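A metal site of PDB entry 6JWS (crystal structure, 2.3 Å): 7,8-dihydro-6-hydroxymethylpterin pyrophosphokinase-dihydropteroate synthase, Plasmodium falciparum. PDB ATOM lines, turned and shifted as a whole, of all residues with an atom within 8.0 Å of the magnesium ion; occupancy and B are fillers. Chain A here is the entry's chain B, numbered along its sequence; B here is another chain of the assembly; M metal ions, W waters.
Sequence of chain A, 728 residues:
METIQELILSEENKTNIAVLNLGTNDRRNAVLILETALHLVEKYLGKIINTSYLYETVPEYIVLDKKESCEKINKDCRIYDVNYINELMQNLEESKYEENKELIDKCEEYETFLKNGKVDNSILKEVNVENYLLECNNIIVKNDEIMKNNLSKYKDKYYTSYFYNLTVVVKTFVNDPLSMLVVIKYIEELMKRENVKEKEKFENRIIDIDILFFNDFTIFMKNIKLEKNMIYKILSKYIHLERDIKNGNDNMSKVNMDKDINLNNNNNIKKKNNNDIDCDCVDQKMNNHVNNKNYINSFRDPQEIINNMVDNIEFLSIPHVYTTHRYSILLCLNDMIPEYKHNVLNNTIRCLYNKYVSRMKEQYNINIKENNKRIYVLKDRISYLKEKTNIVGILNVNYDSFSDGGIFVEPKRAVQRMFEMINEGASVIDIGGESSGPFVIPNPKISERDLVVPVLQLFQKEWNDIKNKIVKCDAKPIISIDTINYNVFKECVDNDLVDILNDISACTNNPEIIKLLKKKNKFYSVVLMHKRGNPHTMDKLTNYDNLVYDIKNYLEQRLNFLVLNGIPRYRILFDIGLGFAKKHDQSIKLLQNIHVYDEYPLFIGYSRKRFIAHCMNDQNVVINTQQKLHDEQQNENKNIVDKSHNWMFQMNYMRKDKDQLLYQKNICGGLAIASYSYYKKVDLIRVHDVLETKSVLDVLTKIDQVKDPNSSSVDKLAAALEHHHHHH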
ATOM      1  N   ARG A 417       5.235 -17.998  14.026  1.00  0.00           N
ATOM      2  CA  ARG A 417       5.556 -19.150  14.857  1.00  0.00           C
ATOM      3  C   ARG A 417       6.951 -19.009  15.473  1.00  0.00           C
ATOM      4  O   ARG A 417       7.128 -19.319  16.641  1.00  0.00           O
ATOM      5  CB  ARG A 417       5.383 -20.446  14.059  1.00  0.00           C
ATOM      6  CG  ARG A 417       5.626 -21.719  14.854  1.00  0.00           C
ATOM      7  CD  ARG A 417       4.719 -21.943  16.046  1.00  0.00           C
ATOM      8  NE  ARG A 417       5.111 -23.149  16.782  1.00  0.00           N
ATOM      9  CZ  ARG A 417       5.139 -23.274  18.109  1.00  0.00           C
ATOM     10  NH1 ARG A 417       4.798 -22.258  18.888  1.00  0.00           N
ATOM     11  NH2 ARG A 417       5.525 -24.415  18.654  1.00  0.00           N
ATOM     12  N   GLU A 424       8.180 -17.912  23.954  1.00  0.00           N
ATOM     13  CA  GLU A 424       7.895 -19.043  24.827  1.00  0.00           C
ATOM     14  C   GLU A 424       9.156 -19.512  25.557  1.00  0.00           C
ATOM     15  O   GLU A 424       9.056 -20.287  26.503  1.00  0.00           O
ATOM     16  CB  GLU A 424       7.152 -20.156  24.087  1.00  0.00           C
ATOM     17  CG  GLU A 424       5.650 -19.949  23.952  1.00  0.00           C
ATOM     18  CD  GLU A 424       5.001 -20.986  23.039  1.00  0.00           C
ATOM     19  OE1 GLU A 424       5.691 -21.952  22.640  1.00  0.00           O
ATOM     20  OE2 GLU A 424       3.788 -20.867  22.731  1.00  0.00           O
ATOM     21  N   ARG A 608       7.968 -35.854  20.433  1.00  0.00           N
ATOM     22  CA  ARG A 608       6.818 -36.416  19.751  1.00  0.00           C
ATOM     23  C   ARG A 608       7.190 -37.663  18.958  1.00  0.00           C
ATOM     24  O   ARG A 608       6.469 -38.017  18.049  1.00  0.00           O
ATOM     25  CB  ARG A 608       6.119 -35.377  18.878  1.00  0.00           C
ATOM     26  CG  ARG A 608       5.440 -34.257  19.670  1.00  0.00           C
ATOM     27  CD  ARG A 608       4.710 -33.342  18.713  1.00  0.00           C
ATOM     28  NE  ARG A 608       4.125 -32.203  19.419  1.00  0.00           N
ATOM     29  CZ  ARG A 608       3.463 -31.193  18.841  1.00  0.00           C
ATOM     30  NH1 ARG A 608       3.281 -31.193  17.522  1.00  0.00           N
ATOM     31  NH2 ARG A 608       2.982 -30.190  19.556  1.00  0.00           N
ATOM     32  N   ASN A 646      -6.319 -29.713  29.435  1.00  0.00           N
ATOM     33  CA  ASN A 646      -5.777 -28.586  28.708  1.00  0.00           C
ATOM     34  C   ASN A 646      -4.841 -29.133  27.618  1.00  0.00           C
ATOM     35  O   ASN A 646      -3.709 -29.513  27.929  1.00  0.00           O
ATOM     36  CB  ASN A 646      -5.092 -27.612  29.669  1.00  0.00           C
ATOM     37  CG  ASN A 646      -4.513 -26.378  29.016  1.00  0.00           C
ATOM     38  OD1 ASN A 646      -4.880 -25.260  29.364  1.00  0.00           O
ATOM     39  ND2 ASN A 646      -3.596 -26.557  28.072  1.00  0.00           N
ATOM     40  N   TRP A 647      -5.321 -29.177  26.364  1.00  0.00           N
ATOM     41  CA  TRP A 647      -4.639 -29.857  25.277  1.00  0.00           C
ATOM     42  C   TRP A 647      -3.349 -29.136  24.902  1.00  0.00           C
ATOM     43  O   TRP A 647      -3.336 -27.927  24.691  1.00  0.00           O
ATOM     44  CB  TRP A 647      -5.538 -30.011  24.036  1.00  0.00           C
ATOM     45  CG  TRP A 647      -6.822 -30.747  24.247  1.00  0.00           C
ATOM     46  CD1 TRP A 647      -8.084 -30.238  24.105  1.00  0.00           C
ATOM     47  CD2 TRP A 647      -6.985 -32.122  24.620  1.00  0.00           C
ATOM     48  NE1 TRP A 647      -9.021 -31.193  24.366  1.00  0.00           N
ATOM     49  CE2 TRP A 647      -8.382 -32.370  24.686  1.00  0.00           C
ATOM     50  CE3 TRP A 647      -6.100 -33.169  24.916  1.00  0.00           C
ATOM     51  CZ2 TRP A 647      -8.902 -33.621  25.025  1.00  0.00           C
ATOM     52  CZ3 TRP A 647      -6.623 -34.409  25.245  1.00  0.00           C
ATOM     53  CH2 TRP A 647      -7.996 -34.628  25.295  1.00  0.00           C
ATOM     54  N   MET A 648      -2.279 -29.921  24.783  1.00  0.00           N
ATOM     55  CA  MET A 648      -0.971 -29.375  24.449  1.00  0.00           C
ATOM     56  C   MET A 648      -0.669 -29.576  22.967  1.00  0.00           C
ATOM     57  O   MET A 648       0.257 -28.949  22.442  1.00  0.00           O
ATOM     58  CB  MET A 648       0.110 -30.008  25.329  1.00  0.00           C
ATOM     59  CG  MET A 648      -0.062 -29.742  26.828  1.00  0.00           C
ATOM     60  SD  MET A 648       0.929 -30.868  27.863  1.00  0.00           S
ATOM     61  CE  MET A 648       0.411 -32.457  27.232  1.00  0.00           C
ATOM     62  N   PHE A 649      -1.454 -30.415  22.288  1.00  0.00           N
ATOM     63  CA  PHE A 649      -1.369 -30.538  20.836  1.00  0.00           C
ATOM     64  C   PHE A 649      -2.403 -29.617  20.189  1.00  0.00           C
ATOM     65  O   PHE A 649      -3.612 -29.805  20.371  1.00  0.00           O
ATOM     66  CB  PHE A 649      -1.533 -32.001  20.413  1.00  0.00           C
ATOM     67  CG  PHE A 649      -1.484 -32.257  18.923  1.00  0.00           C
ATOM     68  CD1 PHE A 649      -0.369 -31.927  18.161  1.00  0.00           C
ATOM     69  CD2 PHE A 649      -2.553 -32.875  18.275  1.00  0.00           C
ATOM     70  CE1 PHE A 649      -0.328 -32.187  16.804  1.00  0.00           C
ATOM     71  CE2 PHE A 649      -2.506 -33.140  16.912  1.00  0.00           C
ATOM     72  CZ  PHE A 649      -1.397 -32.789  16.174  1.00  0.00           C
ATOM     73  N   GLN A 650      -1.925 -28.614  19.439  1.00  0.00           N
ATOM     74  CA  GLN A 650      -2.774 -27.763  18.610  1.00  0.00           C
ATOM     75  C   GLN A 650      -3.076 -28.490  17.308  1.00  0.00           C
ATOM     76  O   GLN A 650      -2.211 -28.594  16.446  1.00  0.00           O
ATOM     77  CB  GLN A 650      -2.102 -26.421  18.302  1.00  0.00           C
ATOM     78  CG  GLN A 650      -1.828 -25.570  19.533  1.00  0.00           C
ATOM     79  CD  GLN A 650      -2.044 -24.088  19.271  1.00  0.00           C
ATOM     80  OE1 GLN A 650      -1.580 -23.536  18.272  1.00  0.00           O
ATOM     81  NE2 GLN A 650      -2.755 -23.445  20.179  1.00  0.00           N
ATOM     82  N   GLN A 664      -1.686 -36.043  23.752  1.00  0.00           N
ATOM     83  CA  GLN A 664      -1.483 -35.488  25.083  1.00  0.00           C
ATOM     84  C   GLN A 664      -0.437 -36.318  25.824  1.00  0.00           C
ATOM     85  O   GLN A 664       0.521 -35.769  26.352  1.00  0.00           O
ATOM     86  CB  GLN A 664      -2.823 -35.398  25.823  1.00  0.00           C
ATOM     87  CG  GLN A 664      -2.746 -34.627  27.142  1.00  0.00           C
ATOM     88  CD  GLN A 664      -2.748 -33.128  26.973  1.00  0.00           C
ATOM     89  OE1 GLN A 664      -2.512 -32.605  25.892  1.00  0.00           O
ATOM     90  NE2 GLN A 664      -3.037 -32.415  28.054  1.00  0.00           N
ATOM     91  N   ILE A 667       3.104 -35.763  24.318  1.00  0.00           N
ATOM     92  CA  ILE A 667       3.753 -34.506  24.689  1.00  0.00           C
ATOM     93  C   ILE A 667       4.139 -34.488  26.168  1.00  0.00           C
ATOM     94  O   ILE A 667       5.230 -34.018  26.506  1.00  0.00           O
ATOM     95  CB  ILE A 667       2.868 -33.315  24.285  1.00  0.00           C
ATOM     96  CG1 ILE A 667       2.726 -33.252  22.772  1.00  0.00           C
ATOM     97  CG2 ILE A 667       3.397 -32.014  24.868  1.00  0.00           C
ATOM     98  CD1 ILE A 667       1.513 -32.445  22.329  1.00  0.00           C
ATOM     99  N   HIS A 688       9.017 -29.517  19.953  1.00  0.00           N
ATOM    100  CA  HIS A 688       7.896 -28.804  19.356  1.00  0.00           C
ATOM    101  C   HIS A 688       7.178 -27.923  20.384  1.00  0.00           C
ATOM    102  O   HIS A 688       6.566 -26.924  20.024  1.00  0.00           O
ATOM    103  CB  HIS A 688       6.853 -29.774  18.798  1.00  0.00           C
ATOM    104  CG  HIS A 688       7.365 -30.682  17.737  1.00  0.00           C
ATOM    105  ND1 HIS A 688       7.948 -31.907  18.030  1.00  0.00           N
ATOM    106  CD2 HIS A 688       7.369 -30.559  16.379  1.00  0.00           C
ATOM    107  CE1 HIS A 688       8.272 -32.512  16.898  1.00  0.00           C
ATOM    108  NE2 HIS A 688       7.944 -31.703  15.879  1.00  0.00           N
ATOM    109  N   ASP A 689       7.212 -28.313  21.657  1.00  0.00           N
ATOM    110  CA  ASP A 689       6.341 -27.739  22.677  1.00  0.00           C
ATOM    111  C   ASP A 689       7.198 -26.868  23.603  1.00  0.00           C
ATOM    112  O   ASP A 689       7.640 -27.320  24.650  1.00  0.00           O
ATOM    113  CB  ASP A 689       5.520 -28.839  23.342  1.00  0.00           C
ATOM    114  CG  ASP A 689       4.661 -29.643  22.363  1.00  0.00           C
ATOM    115  OD1 ASP A 689       3.584 -29.149  21.983  1.00  0.00           O
ATOM    116  OD2 ASP A 689       5.069 -30.792  21.981  1.00  0.00           O
ATOM    117  N   VAL A 690       7.434 -25.615  23.187  1.00  0.00           N
ATOM    118  CA  VAL A 690       8.437 -24.761  23.798  1.00  0.00           C
ATOM    119  C   VAL A 690       7.917 -24.255  25.154  1.00  0.00           C
ATOM    120  O   VAL A 690       8.651 -24.296  26.142  1.00  0.00           O
ATOM    121  CB  VAL A 690       8.859 -23.603  22.870  1.00  0.00           C
ATOM    122  CG1 VAL A 690       9.797 -22.637  23.585  1.00  0.00           C
ATOM    123  CG2 VAL A 690       9.488 -24.080  21.571  1.00  0.00           C
ATOM    124  N   LEU A 691       6.647 -23.795  25.193  1.00  0.00           N
ATOM    125  CA  LEU A 691       6.086 -23.226  26.406  1.00  0.00           C
ATOM    126  C   LEU A 691       6.053 -24.304  27.485  1.00  0.00           C
ATOM    127  O   LEU A 691       6.375 -24.051  28.643  1.00  0.00           O
ATOM    128  CB  LEU A 691       4.678 -22.684  26.146  1.00  0.00           C
ATOM    129  CG  LEU A 691       3.912 -22.243  27.385  1.00  0.00           C
ATOM    130  CD1 LEU A 691       2.992 -21.053  27.073  1.00  0.00           C
ATOM    131  CD2 LEU A 691       3.136 -23.412  28.019  1.00  0.00           C
ATOM    132  N   GLU A 692       5.631 -25.510  27.103  1.00  0.00           N
ATOM    133  CA  GLU A 692       5.514 -26.605  28.047  1.00  0.00           C
ATOM    134  C   GLU A 692       6.889 -26.944  28.627  1.00  0.00           C
ATOM    135  O   GLU A 692       7.057 -27.087  29.828  1.00  0.00           O
ATOM    136  CB  GLU A 692       4.883 -27.807  27.333  1.00  0.00           C
ATOM    137  CG  GLU A 692       3.466 -27.543  26.819  1.00  0.00           C
ATOM    138  CD  GLU A 692       3.342 -27.031  25.394  1.00  0.00           C
ATOM    139  OE1 GLU A 692       4.072 -26.082  25.007  1.00  0.00           O
ATOM    140  OE2 GLU A 692       2.516 -27.588  24.637  1.00  0.00           O
ATOM    141  N   THR A 693       7.895 -27.070  27.750  1.00  0.00           N
ATOM    142  CA  THR A 693       9.239 -27.484  28.131  1.00  0.00           C
ATOM    143  C   THR A 693       9.875 -26.440  29.043  1.00  0.00           C
ATOM    144  O   THR A 693      10.493 -26.773  30.061  1.00  0.00           O
ATOM    145  CB  THR A 693      10.080 -27.782  26.880  1.00  0.00           C
ATOM    146  OG1 THR A 693       9.377 -28.762  26.104  1.00  0.00           O
ATOM    147  CG2 THR A 693      11.472 -28.276  27.195  1.00  0.00           C
ATOM    148  N   GLN B 664      -1.812 -23.514  31.403  1.00  0.00           N
ATOM    149  CA  GLN B 664      -1.001 -24.566  30.809  1.00  0.00           C
ATOM    150  C   GLN B 664       0.373 -24.599  31.476  1.00  0.00           C
ATOM    151  O   GLN B 664       0.850 -25.673  31.808  1.00  0.00           O
ATOM    152  CB  GLN B 664      -0.940 -24.453  29.280  1.00  0.00           C
ATOM    153  CG  GLN B 664      -0.194 -25.633  28.650  1.00  0.00           C
ATOM    154  CD  GLN B 664      -0.410 -25.768  27.162  1.00  0.00           C
ATOM    155  OE1 GLN B 664      -0.999 -26.736  26.687  1.00  0.00           O
ATOM    156  NE2 GLN B 664       0.051 -24.780  26.410  1.00  0.00           N
ATOM    157  N   CYS B 668       2.069 -27.678  33.391  1.00  0.00           N
ATOM    158  CA  CYS B 668       3.362 -28.167  32.970  1.00  0.00           C
ATOM    159  C   CYS B 668       4.377 -28.056  34.116  1.00  0.00           C
ATOM    160  O   CYS B 668       5.171 -28.980  34.303  1.00  0.00           O
ATOM    161  CB  CYS B 668       3.829 -27.524  31.680  1.00  0.00           C
ATOM    162  SG  CYS B 668       2.763 -27.962  30.281  1.00  0.00           S
HETATM  163 MG    MG M   1       2.008 -27.564  22.509  1.00  0.00          MG
HETATM  164  O   HOH W   1       0.168 -26.196  23.213  1.00  0.00           O
HETATM  165  O   HOH W   2       3.267 -25.811  22.773  1.00  0.00           O
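N of Met 648 lies within hydrogen-bond range of OE1 of Gln 664 of chain A, 2.9 Å away. The side-chain carboxylate of Asp 689 lies within salt-bridge range of the guanidinium group of Arg 608. OG1 of Thr 693 is in hydrogen-bond range of O of Asp 689 (2.7 Å).
The magnesium ion is bound by water W2 (2.2 Å), OE2 of Glu 692 (2.2 Å), O of Met 648 (2.2 Å), OD1 of Asp 689 (2.3 Å) and water W1 (2.4 Å).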
